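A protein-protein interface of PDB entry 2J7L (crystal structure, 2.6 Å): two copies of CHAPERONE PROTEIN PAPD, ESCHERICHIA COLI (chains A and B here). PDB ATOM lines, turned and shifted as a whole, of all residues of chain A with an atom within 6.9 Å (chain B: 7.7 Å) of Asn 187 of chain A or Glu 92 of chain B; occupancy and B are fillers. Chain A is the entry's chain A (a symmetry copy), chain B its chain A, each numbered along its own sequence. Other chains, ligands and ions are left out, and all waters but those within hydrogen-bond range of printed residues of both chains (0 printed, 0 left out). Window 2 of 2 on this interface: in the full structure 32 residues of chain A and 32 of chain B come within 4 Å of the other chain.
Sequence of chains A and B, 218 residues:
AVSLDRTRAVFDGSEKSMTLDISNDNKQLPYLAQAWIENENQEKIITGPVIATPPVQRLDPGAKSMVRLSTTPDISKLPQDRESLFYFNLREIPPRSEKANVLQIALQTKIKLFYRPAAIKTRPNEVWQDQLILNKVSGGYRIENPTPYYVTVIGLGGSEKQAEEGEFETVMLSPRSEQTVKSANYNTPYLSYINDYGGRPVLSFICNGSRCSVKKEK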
ATOM      1  N   LYS A 136     -26.172 -26.770  -4.347  1.00  0.00           N
ATOM      2  CA  LYS A 136     -25.215 -27.502  -3.534  1.00  0.00           C
ATOM      3  C   LYS A 136     -24.272 -28.319  -4.407  1.00  0.00           C
ATOM      4  O   LYS A 136     -24.693 -28.982  -5.354  1.00  0.00           O
ATOM      5  CB  LYS A 136     -25.934 -28.436  -2.560  1.00  0.00           C
ATOM      6  CG  LYS A 136     -27.053 -27.786  -1.762  1.00  0.00           C
ATOM      7  CD  LYS A 136     -27.508 -28.666  -0.597  1.00  0.00           C
ATOM      8  CE  LYS A 136     -28.613 -27.992   0.220  1.00  0.00           C
ATOM      9  NZ  LYS A 136     -28.847 -28.677   1.530  1.00  0.00           N
ATOM     10  N   TYR A 141     -21.317 -24.013  -3.163  1.00  0.00           N
ATOM     11  CA  TYR A 141     -22.520 -23.879  -3.969  1.00  0.00           C
ATOM     12  C   TYR A 141     -22.169 -23.366  -5.354  1.00  0.00           C
ATOM     13  O   TYR A 141     -21.083 -22.826  -5.577  1.00  0.00           O
ATOM     14  CB  TYR A 141     -23.514 -22.901  -3.336  1.00  0.00           C
ATOM     15  CG  TYR A 141     -23.957 -23.270  -1.950  1.00  0.00           C
ATOM     16  CD1 TYR A 141     -23.186 -22.938  -0.848  1.00  0.00           C
ATOM     17  CD2 TYR A 141     -25.136 -23.978  -1.741  1.00  0.00           C
ATOM     18  CE1 TYR A 141     -23.571 -23.301   0.435  1.00  0.00           C
ATOM     19  CE2 TYR A 141     -25.537 -24.351  -0.458  1.00  0.00           C
ATOM     20  CZ  TYR A 141     -24.750 -24.006   0.631  1.00  0.00           C
ATOM     21  OH  TYR A 141     -25.141 -24.340   1.915  1.00  0.00           O
ATOM     22  N   GLY A 158     -24.947 -19.874   7.720  1.00  0.00           N
ATOM     23  CA  GLY A 158     -26.059 -20.711   8.132  1.00  0.00           C
ATOM     24  C   GLY A 158     -27.106 -19.931   8.901  1.00  0.00           C
ATOM     25  O   GLY A 158     -28.167 -20.465   9.222  1.00  0.00           O
ATOM     26  N   ALA A 184     -19.541 -24.050   3.526  1.00  0.00           N
ATOM     27  CA  ALA A 184     -19.929 -25.247   4.264  1.00  0.00           C
ATOM     28  C   ALA A 184     -21.393 -25.480   3.876  1.00  0.00           C
ATOM     29  O   ALA A 184     -22.062 -24.551   3.408  1.00  0.00           O
ATOM     30  CB  ALA A 184     -19.808 -25.004   5.764  1.00  0.00           C
ATOM     31  N   ASN A 185     -21.880 -26.707   4.055  1.00  0.00           N
ATOM     32  CA  ASN A 185     -23.265 -27.042   3.718  1.00  0.00           C
ATOM     33  C   ASN A 185     -24.209 -26.587   4.829  1.00  0.00           C
ATOM     34  O   ASN A 185     -24.244 -27.162   5.908  1.00  0.00           O
ATOM     35  CB  ASN A 185     -23.386 -28.556   3.484  1.00  0.00           C
ATOM     36  CG  ASN A 185     -24.796 -28.988   3.145  1.00  0.00           C
ATOM     37  OD1 ASN A 185     -25.485 -28.342   2.350  1.00  0.00           O
ATOM     38  ND2 ASN A 185     -25.229 -30.098   3.736  1.00  0.00           N
ATOM     39  N   TYR A 186     -24.984 -25.550   4.553  1.00  0.00           N
ATOM     40  CA  TYR A 186     -25.885 -24.998   5.551  1.00  0.00           C
ATOM     41  C   TYR A 186     -27.344 -25.402   5.414  1.00  0.00           C
ATOM     42  O   TYR A 186     -27.921 -25.356   4.325  1.00  0.00           O
ATOM     43  CB  TYR A 186     -25.777 -23.475   5.533  1.00  0.00           C
ATOM     44  CG  TYR A 186     -24.428 -22.970   5.981  1.00  0.00           C
ATOM     45  CD1 TYR A 186     -23.701 -22.070   5.200  1.00  0.00           C
ATOM     46  CD2 TYR A 186     -23.885 -23.370   7.199  1.00  0.00           C
ATOM     47  CE1 TYR A 186     -22.469 -21.578   5.623  1.00  0.00           C
ATOM     48  CE2 TYR A 186     -22.652 -22.883   7.630  1.00  0.00           C
ATOM     49  CZ  TYR A 186     -21.951 -21.987   6.839  1.00  0.00           C
ATOM     50  OH  TYR A 186     -20.747 -21.496   7.277  1.00  0.00           O
ATOM     51  N   ASN A 187     -27.939 -25.783   6.537  1.00  0.00           N
ATOM     52  CA  ASN A 187     -29.336 -26.183   6.564  1.00  0.00           C
ATOM     53  C   ASN A 187     -30.229 -25.136   5.884  1.00  0.00           C
ATOM     54  O   ASN A 187     -30.951 -25.434   4.936  1.00  0.00           O
ATOM     55  CB  ASN A 187     -29.778 -26.358   8.012  1.00  0.00           C
ATOM     56  CG  ASN A 187     -31.109 -27.039   8.132  1.00  0.00           C
ATOM     57  OD1 ASN A 187     -31.797 -26.882   9.133  1.00  0.00           O
ATOM     58  ND2 ASN A 187     -31.480 -27.811   7.117  1.00  0.00           N
ATOM     59  N   THR A 188     -30.183 -23.915   6.406  1.00  0.00           N
ATOM     60  CA  THR A 188     -30.950 -22.800   5.868  1.00  0.00           C
ATOM     61  C   THR A 188     -29.989 -21.654   5.531  1.00  0.00           C
ATOM     62  O   THR A 188     -29.743 -20.756   6.346  1.00  0.00           O
ATOM     63  CB  THR A 188     -32.048 -22.321   6.875  1.00  0.00           C
ATOM     64  OG1 THR A 188     -31.450 -21.885   8.108  1.00  0.00           O
ATOM     65  CG2 THR A 188     -33.026 -23.447   7.149  1.00  0.00           C
ATOM     66  N   PRO A 189     -29.429 -21.678   4.307  1.00  0.00           N
ATOM     67  CA  PRO A 189     -28.477 -20.676   3.798  1.00  0.00           C
ATOM     68  C   PRO A 189     -28.951 -19.215   3.826  1.00  0.00           C
ATOM     69  O   PRO A 189     -30.090 -18.904   3.474  1.00  0.00           O
ATOM     70  CB  PRO A 189     -28.205 -21.153   2.368  1.00  0.00           C
ATOM     71  CG  PRO A 189     -28.412 -22.631   2.447  1.00  0.00           C
ATOM     72  CD  PRO A 189     -29.646 -22.743   3.308  1.00  0.00           C
ATOM     73  N   PHE A 205     -32.627 -18.150   2.424  1.00  0.00           N
ATOM     74  CA  PHE A 205     -32.908 -19.215   1.469  1.00  0.00           C
ATOM     75  C   PHE A 205     -33.444 -20.485   2.134  1.00  0.00           C
ATOM     76  O   PHE A 205     -33.291 -20.686   3.344  1.00  0.00           O
ATOM     77  CB  PHE A 205     -31.646 -19.579   0.687  1.00  0.00           C
ATOM     78  CG  PHE A 205     -31.337 -18.653  -0.454  1.00  0.00           C
ATOM     79  CD1 PHE A 205     -31.255 -17.280  -0.259  1.00  0.00           C
ATOM     80  CD2 PHE A 205     -31.072 -19.164  -1.717  1.00  0.00           C
ATOM     81  CE1 PHE A 205     -30.906 -16.430  -1.306  1.00  0.00           C
ATOM     82  CE2 PHE A 205     -30.724 -18.327  -2.767  1.00  0.00           C
ATOM     83  CZ  PHE A 205     -30.639 -16.956  -2.562  1.00  0.00           C
ATOM     84  N   ILE A 206     -34.057 -21.336   1.309  1.00  0.00           N
ATOM     85  CA  ILE A 206     -34.639 -22.616   1.723  1.00  0.00           C
ATOM     86  C   ILE A 206     -34.276 -23.649   0.668  1.00  0.00           C
ATOM     87  O   ILE A 206     -34.467 -23.418  -0.523  1.00  0.00           O
ATOM     88  CB  ILE A 206     -36.188 -22.534   1.823  1.00  0.00           C
ATOM     89  CG1 ILE A 206     -36.583 -21.609   2.974  1.00  0.00           C
ATOM     90  CG2 ILE A 206     -36.784 -23.923   1.980  1.00  0.00           C
ATOM     91  CD1 ILE A 206     -35.969 -21.993   4.313  1.00  0.00           C
ATOM     92  N   CYS A 207     -33.760 -24.792   1.094  1.00  0.00           N
ATOM     93  CA  CYS A 207     -33.365 -25.793   0.124  1.00  0.00           C
ATOM     94  C   CYS A 207     -34.357 -26.918  -0.084  1.00  0.00           C
ATOM     95  O   CYS A 207     -35.306 -27.091   0.678  1.00  0.00           O
ATOM     96  CB  CYS A 207     -32.010 -26.382   0.505  1.00  0.00           C
ATOM     97  SG  CYS A 207     -30.696 -25.141   0.725  1.00  0.00           S
ATOM     98  N   CYS A 212     -31.500 -24.488  -3.847  1.00  0.00           N
ATOM     99  CA  CYS A 212     -32.026 -23.651  -2.773  1.00  0.00           C
ATOM    100  C   CYS A 212     -32.508 -22.364  -3.392  1.00  0.00           C
ATOM    101  O   CYS A 212     -31.859 -21.822  -4.279  1.00  0.00           O
ATOM    102  CB  CYS A 212     -30.953 -23.332  -1.738  1.00  0.00           C
ATOM    103  SG  CYS A 212     -30.008 -24.774  -1.156  1.00  0.00           S
ATOM    104  N   ALA B   1     -33.723 -23.815  13.330  1.00  0.00           N
ATOM    105  CA  ALA B   1     -34.325 -23.566  14.677  1.00  0.00           C
ATOM    106  C   ALA B   1     -33.265 -23.330  15.743  1.00  0.00           C
ATOM    107  O   ALA B   1     -33.337 -22.376  16.515  1.00  0.00           O
ATOM    108  CB  ALA B   1     -35.193 -24.746  15.082  1.00  0.00           C
ATOM    109  N   VAL B   2     -32.292 -24.229  15.794  1.00  0.00           N
ATOM    110  CA  VAL B   2     -31.210 -24.139  16.758  1.00  0.00           C
ATOM    111  C   VAL B   2     -30.199 -23.129  16.250  1.00  0.00           C
ATOM    112  O   VAL B   2     -29.802 -23.179  15.092  1.00  0.00           O
ATOM    113  CB  VAL B   2     -30.532 -25.493  16.913  1.00  0.00           C
ATOM    114  CG1 VAL B   2     -29.482 -25.423  17.989  1.00  0.00           C
ATOM    115  CG2 VAL B   2     -31.577 -26.545  17.232  1.00  0.00           C
ATOM    116  N   SER B   3     -29.784 -22.214  17.115  1.00  0.00           N
ATOM    117  CA  SER B   3     -28.839 -21.188  16.726  1.00  0.00           C
ATOM    118  C   SER B   3     -27.732 -21.009  17.764  1.00  0.00           C
ATOM    119  O   SER B   3     -27.869 -21.445  18.902  1.00  0.00           O
ATOM    120  CB  SER B   3     -29.591 -19.888  16.543  1.00  0.00           C
ATOM    121  OG  SER B   3     -30.318 -19.599  17.724  1.00  0.00           O
ATOM    122  N   SER B  23     -29.886 -21.906  21.399  1.00  0.00           N
ATOM    123  CA  SER B  23     -31.323 -21.774  21.623  1.00  0.00           C
ATOM    124  C   SER B  23     -32.181 -22.330  20.494  1.00  0.00           C
ATOM    125  O   SER B  23     -31.771 -22.383  19.331  1.00  0.00           O
ATOM    126  CB  SER B  23     -31.706 -20.310  21.846  1.00  0.00           C
ATOM    127  OG  SER B  23     -31.807 -19.614  20.617  1.00  0.00           O
ATOM    128  N   ASN B  24     -33.386 -22.748  20.867  1.00  0.00           N
ATOM    129  CA  ASN B  24     -34.343 -23.287  19.916  1.00  0.00           C
ATOM    130  C   ASN B  24     -35.362 -22.203  19.645  1.00  0.00           C
ATOM    131  O   ASN B  24     -36.347 -22.067  20.360  1.00  0.00           O
ATOM    132  CB  ASN B  24     -35.032 -24.518  20.488  1.00  0.00           C
ATOM    133  CG  ASN B  24     -36.116 -25.038  19.587  1.00  0.00           C
ATOM    134  OD1 ASN B  24     -36.078 -24.839  18.376  1.00  0.00           O
ATOM    135  ND2 ASN B  24     -37.088 -25.727  20.169  1.00  0.00           N
ATOM    136  N   ASP B  25     -35.107 -21.426  18.604  1.00  0.00           N
ATOM    137  CA  ASP B  25     -35.985 -20.335  18.249  1.00  0.00           C
ATOM    138  C   ASP B  25     -37.372 -20.804  17.861  1.00  0.00           C
ATOM    139  O   ASP B  25     -38.274 -19.993  17.680  1.00  0.00           O
ATOM    140  CB  ASP B  25     -35.345 -19.533  17.130  1.00  0.00           C
ATOM    141  CG  ASP B  25     -33.901 -19.199  17.434  1.00  0.00           C
ATOM    142  OD1 ASP B  25     -33.643 -18.698  18.552  1.00  0.00           O
ATOM    143  OD2 ASP B  25     -33.034 -19.442  16.563  1.00  0.00           O
ATOM    144  N   ASN B  26     -37.548 -22.111  17.743  1.00  0.00           N
ATOM    145  CA  ASN B  26     -38.850 -22.651  17.396  1.00  0.00           C
ATOM    146  C   ASN B  26     -39.674 -22.804  18.683  1.00  0.00           C
ATOM    147  O   ASN B  26     -39.357 -23.633  19.531  1.00  0.00           O
ATOM    148  CB  ASN B  26     -38.683 -23.997  16.705  1.00  0.00           C
ATOM    149  CG  ASN B  26     -39.956 -24.468  16.057  1.00  0.00           C
ATOM    150  OD1 ASN B  26     -41.015 -24.453  16.668  1.00  0.00           O
ATOM    151  ND2 ASN B  26     -39.860 -24.889  14.808  1.00  0.00           N
ATOM    152  N   TYR B  31     -36.329 -29.598  19.170  1.00  0.00           N
ATOM    153  CA  TYR B  31     -35.226 -29.918  18.263  1.00  0.00           C
ATOM    154  C   TYR B  31     -34.026 -30.499  19.015  1.00  0.00           C
ATOM    155  O   TYR B  31     -33.918 -30.368  20.234  1.00  0.00           O
ATOM    156  CB  TYR B  31     -34.765 -28.656  17.508  1.00  0.00           C
ATOM    157  CG  TYR B  31     -35.503 -28.345  16.214  1.00  0.00           C
ATOM    158  CD1 TYR B  31     -36.804 -27.831  16.221  1.00  0.00           C
ATOM    159  CD2 TYR B  31     -34.891 -28.560  14.978  1.00  0.00           C
ATOM    160  CE1 TYR B  31     -37.474 -27.540  15.021  1.00  0.00           C
ATOM    161  CE2 TYR B  31     -35.546 -28.276  13.782  1.00  0.00           C
ATOM    162  CZ  TYR B  31     -36.835 -27.767  13.807  1.00  0.00           C
ATOM    163  OH  TYR B  31     -37.471 -27.492  12.614  1.00  0.00           O
ATOM    164  N   LEU B  32     -33.124 -31.143  18.284  1.00  0.00           N
ATOM    165  CA  LEU B  32     -31.913 -31.684  18.898  1.00  0.00           C
ATOM    166  C   LEU B  32     -30.722 -30.820  18.464  1.00  0.00           C
ATOM    167  O   LEU B  32     -30.677 -30.336  17.335  1.00  0.00           O
ATOM    168  CB  LEU B  32     -31.690 -33.143  18.485  1.00  0.00           C
ATOM    169  CG  LEU B  32     -32.740 -34.159  18.947  1.00  0.00           C
ATOM    170  CD1 LEU B  32     -32.259 -35.544  18.568  1.00  0.00           C
ATOM    171  CD2 LEU B  32     -32.970 -34.073  20.459  1.00  0.00           C
ATOM    172  N   ALA B  33     -29.782 -30.602  19.378  1.00  0.00           N
ATOM    173  CA  ALA B  33     -28.594 -29.802  19.093  1.00  0.00           C
ATOM    174  C   ALA B  33     -27.376 -30.698  19.124  1.00  0.00           C
ATOM    175  O   ALA B  33     -26.968 -31.202  20.172  1.00  0.00           O
ATOM    176  CB  ALA B  33     -28.431 -28.681  20.118  1.00  0.00           C
ATOM    177  N   GLN B  34     -26.790 -30.896  17.961  1.00  0.00           N
ATOM    178  CA  GLN B  34     -25.618 -31.728  17.871  1.00  0.00           C
ATOM    179  C   GLN B  34     -24.392 -30.842  17.679  1.00  0.00           C
ATOM    180  O   GLN B  34     -24.394 -29.946  16.833  1.00  0.00           O
ATOM    181  CB  GLN B  34     -25.796 -32.668  16.720  1.00  0.00           C
ATOM    182  CG  GLN B  34     -24.723 -33.663  16.596  1.00  0.00           C
ATOM    183  CD  GLN B  34     -25.097 -34.667  15.564  1.00  0.00           C
ATOM    184  OE1 GLN B  34     -25.478 -34.302  14.441  1.00  0.00           O
ATOM    185  NE2 GLN B  34     -25.018 -35.949  15.927  1.00  0.00           N
ATOM    186  N   ALA B  35     -23.348 -31.089  18.466  1.00  0.00           N
ATOM    187  CA  ALA B  35     -22.145 -30.273  18.378  1.00  0.00           C
ATOM    188  C   ALA B  35     -20.870 -31.098  18.329  1.00  0.00           C
ATOM    189  O   ALA B  35     -20.802 -32.175  18.914  1.00  0.00           O
ATOM    190  CB  ALA B  35     -22.092 -29.313  19.563  1.00  0.00           C
ATOM    191  N   TRP B  36     -19.862 -30.595  17.628  1.00  0.00           N
ATOM    192  CA  TRP B  36     -18.577 -31.288  17.562  1.00  0.00           C
ATOM    193  C   TRP B  36     -17.433 -30.388  17.089  1.00  0.00           C
ATOM    194  O   TRP B  36     -17.639 -29.355  16.458  1.00  0.00           O
ATOM    195  CB  TRP B  36     -18.670 -32.544  16.679  1.00  0.00           C
ATOM    196  CG  TRP B  36     -18.803 -32.261  15.227  1.00  0.00           C
ATOM    197  CD1 TRP B  36     -17.791 -32.093  14.318  1.00  0.00           C
ATOM    198  CD2 TRP B  36     -20.022 -32.037  14.521  1.00  0.00           C
ATOM    199  NE1 TRP B  36     -18.309 -31.771  13.088  1.00  0.00           N
ATOM    200  CE2 TRP B  36     -19.676 -31.730  13.179  1.00  0.00           C
ATOM    201  CE3 TRP B  36     -21.378 -32.062  14.891  1.00  0.00           C
ATOM    202  CZ2 TRP B  36     -20.640 -31.445  12.201  1.00  0.00           C
ATOM    203  CZ3 TRP B  36     -22.341 -31.777  13.920  1.00  0.00           C
ATOM    204  CH2 TRP B  36     -21.961 -31.472  12.586  1.00  0.00           C
ATOM    205  N   LEU B  90     -22.334 -27.055  14.708  1.00  0.00           N
ATOM    206  CA  LEU B  90     -23.651 -27.256  15.301  1.00  0.00           C
ATOM    207  C   LEU B  90     -24.691 -27.640  14.243  1.00  0.00           C
ATOM    208  O   LEU B  90     -24.863 -26.943  13.243  1.00  0.00           O
ATOM    209  CB  LEU B  90     -24.082 -25.980  16.024  1.00  0.00           C
ATOM    210  CG  LEU B  90     -25.480 -25.932  16.651  1.00  0.00           C
ATOM    211  CD1 LEU B  90     -25.466 -26.698  17.949  1.00  0.00           C
ATOM    212  CD2 LEU B  90     -25.894 -24.481  16.917  1.00  0.00           C
ATOM    213  N   ARG B  91     -25.355 -28.772  14.461  1.00  0.00           N
ATOM    214  CA  ARG B  91     -26.404 -29.255  13.565  1.00  0.00           C
ATOM    215  C   ARG B  91     -27.687 -29.484  14.365  1.00  0.00           C
ATOM    216  O   ARG B  91     -27.632 -29.926  15.515  1.00  0.00           O
ATOM    217  CB  ARG B  91     -25.997 -30.571  12.893  1.00  0.00           C
ATOM    218  CG  ARG B  91     -27.214 -31.359  12.430  1.00  0.00           C
ATOM    219  CD  ARG B  91     -26.974 -32.237  11.222  1.00  0.00           C
ATOM    220  NE  ARG B  91     -25.931 -33.215  11.472  1.00  0.00           N
ATOM    221  CZ  ARG B  91     -24.683 -33.095  11.038  1.00  0.00           C
ATOM    222  NH1 ARG B  91     -24.334 -32.033  10.322  1.00  0.00           N
ATOM    223  NH2 ARG B  91     -23.780 -34.025  11.329  1.00  0.00           N
ATOM    224  N   GLU B  92     -28.840 -29.194  13.767  1.00  0.00           N
ATOM    225  CA  GLU B  92     -30.113 -29.407  14.463  1.00  0.00           C
ATOM    226  C   GLU B  92     -30.848 -30.612  13.886  1.00  0.00           C
ATOM    227  O   GLU B  92     -30.699 -30.937  12.707  1.00  0.00           O
ATOM    228  CB  GLU B  92     -31.012 -28.172  14.360  1.00  0.00           C
ATOM    229  CG  GLU B  92     -31.678 -27.995  13.001  1.00  0.00           C
ATOM    230  CD  GLU B  92     -32.449 -26.679  12.872  1.00  0.00           C
ATOM    231  OE1 GLU B  92     -33.115 -26.488  11.824  1.00  0.00           O
ATOM    232  OE2 GLU B  92     -32.388 -25.842  13.809  1.00  0.00           O
ATOM    233  N   ILE B  93     -31.616 -31.284  14.741  1.00  0.00           N
ATOM    234  CA  ILE B  93     -32.412 -32.445  14.343  1.00  0.00           C
ATOM    235  C   ILE B  93     -33.848 -32.183  14.761  1.00  0.00           C
ATOM    236  O   ILE B  93     -34.175 -32.185  15.954  1.00  0.00           O
ATOM    237  CB  ILE B  93     -31.927 -33.725  15.021  1.00  0.00           C
ATOM    238  CG1 ILE B  93     -30.450 -33.920  14.723  1.00  0.00           C
ATOM    239  CG2 ILE B  93     -32.701 -34.924  14.495  1.00  0.00           C
ATOM    240  CD1 ILE B  93     -29.888 -35.129  15.371  1.00  0.00           C
ATOM    241  N   PRO B  94     -34.726 -31.945  13.777  1.00  0.00           N
ATOM    242  CA  PRO B  94     -36.154 -31.660  13.964  1.00  0.00           C
ATOM    243  C   PRO B  94     -36.955 -32.851  14.498  1.00  0.00           C
ATOM    244  O   PRO B  94     -36.406 -33.926  14.720  1.00  0.00           O
ATOM    245  CB  PRO B  94     -36.594 -31.267  12.563  1.00  0.00           C
ATOM    246  CG  PRO B  94     -35.795 -32.228  11.725  1.00  0.00           C
ATOM    247  CD  PRO B  94     -34.416 -32.110  12.345  1.00  0.00           C
ATOM    248  N   GLN B 104     -28.196 -36.463   4.042  1.00  0.00           N
ATOM    249  CA  GLN B 104     -27.955 -35.017   3.983  1.00  0.00           C
ATOM    250  C   GLN B 104     -27.421 -34.472   5.319  1.00  0.00           C
ATOM    251  O   GLN B 104     -28.137 -34.437   6.329  1.00  0.00           O
ATOM    252  CB  GLN B 104     -29.248 -34.284   3.602  1.00  0.00           C
ATOM    253  CG  GLN B 104     -29.072 -32.812   3.181  1.00  0.00           C
ATOM    254  CD  GLN B 104     -28.280 -32.624   1.878  1.00  0.00           C
ATOM    255  OE1 GLN B 104     -28.508 -33.325   0.881  1.00  0.00           O
ATOM    256  NE2 GLN B 104     -27.355 -31.669   1.885  1.00  0.00           N
ATOM    257  N   ILE B 105     -26.165 -34.029   5.311  1.00  0.00           N
ATOM    258  CA  ILE B 105     -25.540 -33.511   6.520  1.00  0.00           C
ATOM    259  C   ILE B 105     -25.412 -31.987   6.541  1.00  0.00           C
ATOM    260  O   ILE B 105     -24.319 -31.465   6.404  1.00  0.00           O
ATOM    261  CB  ILE B 105     -24.133 -34.106   6.710  1.00  0.00           C
ATOM    262  CG1 ILE B 105     -24.162 -35.623   6.503  1.00  0.00           C
ATOM    263  CG2 ILE B 105     -23.636 -33.784   8.094  1.00  0.00           C
ATOM    264  CD1 ILE B 105     -24.095 -36.052   5.050  1.00  0.00           C
ATOM    265  N   ALA B 106     -26.519 -31.274   6.726  1.00  0.00           N
ATOM    266  CA  ALA B 106     -26.490 -29.811   6.757  1.00  0.00           C
ATOM    267  C   ALA B 106     -26.258 -29.272   8.165  1.00  0.00           C
ATOM    268  O   ALA B 106     -26.795 -29.798   9.139  1.00  0.00           O
ATOM    269  CB  ALA B 106     -27.792 -29.243   6.192  1.00  0.00           C
ATOM    270  N   LEU B 107     -25.478 -28.204   8.263  1.00  0.00           N
ATOM    271  CA  LEU B 107     -25.172 -27.618   9.554  1.00  0.00           C
ATOM    272  C   LEU B 107     -25.961 -26.369   9.841  1.00  0.00           C
ATOM    273  O   LEU B 107     -26.506 -25.737   8.940  1.00  0.00           O
ATOM    274  CB  LEU B 107     -23.694 -27.255   9.646  1.00  0.00           C
ATOM    275  CG  LEU B 107     -22.667 -28.374   9.686  1.00  0.00           C
ATOM    276  CD1 LEU B 107     -22.815 -29.311   8.496  1.00  0.00           C
ATOM    277  CD2 LEU B 107     -21.307 -27.718   9.682  1.00  0.00           C
ATOM    278  N   GLN B 108     -26.003 -26.010  11.114  1.00  0.00           N
ATOM    279  CA  GLN B 108     -26.697 -24.807  11.525  1.00  0.00           C
ATOM    280  C   GLN B 108     -25.736 -23.644  11.420  1.00  0.00           C
ATOM    281  O   GLN B 108     -26.115 -22.535  11.056  1.00  0.00           O
ATOM    282  CB  GLN B 108     -27.210 -24.954  12.958  1.00  0.00           C
ATOM    283  CG  GLN B 108     -28.461 -25.789  12.992  1.00  0.00           C
ATOM    284  CD  GLN B 108     -29.471 -25.287  11.983  1.00  0.00           C
ATOM    285  OE1 GLN B 108     -30.083 -24.241  12.177  1.00  0.00           O
ATOM    286  NE2 GLN B 108     -29.635 -26.023  10.884  1.00  0.00           N
ATOM    287  N   THR B 109     -24.477 -23.923  11.731  1.00  0.00           N
ATOM    288  CA  THR B 109     -23.426 -22.925  11.666  1.00  0.00           C
ATOM    289  C   THR B 109     -22.075 -23.563  11.969  1.00  0.00           C
ATOM    290  O   THR B 109     -21.980 -24.516  12.740  1.00  0.00           O
ATOM    291  CB  THR B 109     -23.676 -21.778  12.668  1.00  0.00           C
ATOM    292  OG1 THR B 109     -22.685 -20.765  12.484  1.00  0.00           O
ATOM    293  CG2 THR B 109     -23.607 -22.293  14.100  1.00  0.00           C
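Of the 24 printed residues of chain B, 6 touch a printed residue of chain A. Hydrophobic or aromatic side chains of chain B within 4 Å of the printed part of chain A: Ala 106 and Leu 107. Along chain B the printed residues that touch a printed residue of chain A span positions 92 to 108. Among the printed residues, 12 pairs touch across the chains.
Among the printed residues, pairs that only touch across the chains: Asn 187 of chain A with Ala 106 of chain B, Tyr 186 of chain A with Leu 107 of chain B and Tyr 186 of chain A with Ala 106 of chain B.
The backbone NH of Ala 1 of chain B sits at hydrogen-bond distance from the side-chain carboxylate of Glu 92 of chain B, at 2.5 Å. The side-chain hydroxyl of Tyr 141 of chain A is in hydrogen-bond range of the backbone NH of Tyr 186 of chain A, 2.9 Å away. SG of Cys 207 of chain A forms a disulfide with SG of Cys 212 of chain A, 2.0 Å away. OE1 of Gln 108 of chain B lies close to O of Val 2 of chain B (3.1 Å). OD1 of Asn 185 of chain A sits at hydrogen-bond distance from NZ of Lys 136 of chain A. O of Leu 90 of chain B sits at hydrogen-bond distance from N of Gln 108 of chain B (2.6 Å).
No position is printed for both chains.
ND2 of Asn 185 of chain A is in hydrogen-bond range of O of Ile 105 of chain B, at 3.1 Å. O of Leu 107 of chain B lies within hydrogen-bond range of N of Asn 187 of chain A (2.8 Å). The backbone carbonyl oxygen (O) of Gln 108 of chain B sits close to the backbone carbonyl oxygen (O) of Gly 158 of chain A. NE2 of Gln 108 of chain B lies close to OD1 of Asn 187 of chain A, 2.9 Å away. The side-chain amide oxygen (OD1) of Asn 187 of chain A lies close to the side-chain carboxylate (OE1) of Glu 92 of chain B, 3.0 Å away. The backbone NH of Leu 107 of chain B is in hydrogen-bond range of the backbone carbonyl oxygen of Asn 185 of chain A, at 2.9 Å. N of Ala 106 of chain B sits close to ND2 of Asn 185 of chain A. NE2 of Gln 104 of chain B lies close to ND2 of Asn 185 of chain A, 3.2 Å away. NE2 of Gln 104 of chain B sits close to NZ of Lys 136 of chain A (3.4 Å).
Printed residues of chain B within 4 Å of Lys 136 of chain A: Gln 104 (3.4 Å). Of the printed residues of chain B, Asn 185 of chain A touches Gln 104, Ile 105, Ala 106 and Leu 107. Of chain B, only Glu 92 (3.0 Å), Ala 106 (3.4 Å), Leu 107 (2.8 Å) and Gln 108 (2.9 Å) come within 4 Å of Asn 187 of chain A. Trp 36 of chain B touches none of the printed residues of chain A. Glu 92 of chain B touches just one residue of chain A: Asn 187. Of the printed residues of chain A, Ile 105 of chain B touches Asn 185. Of the printed residues of chain A, Ala 106 of chain B touches Asn 185, Tyr 186 and Asn 187. Of the printed residues of chain A, Leu 107 of chain B touches Asn 185, Tyr 186 and Asn 187.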
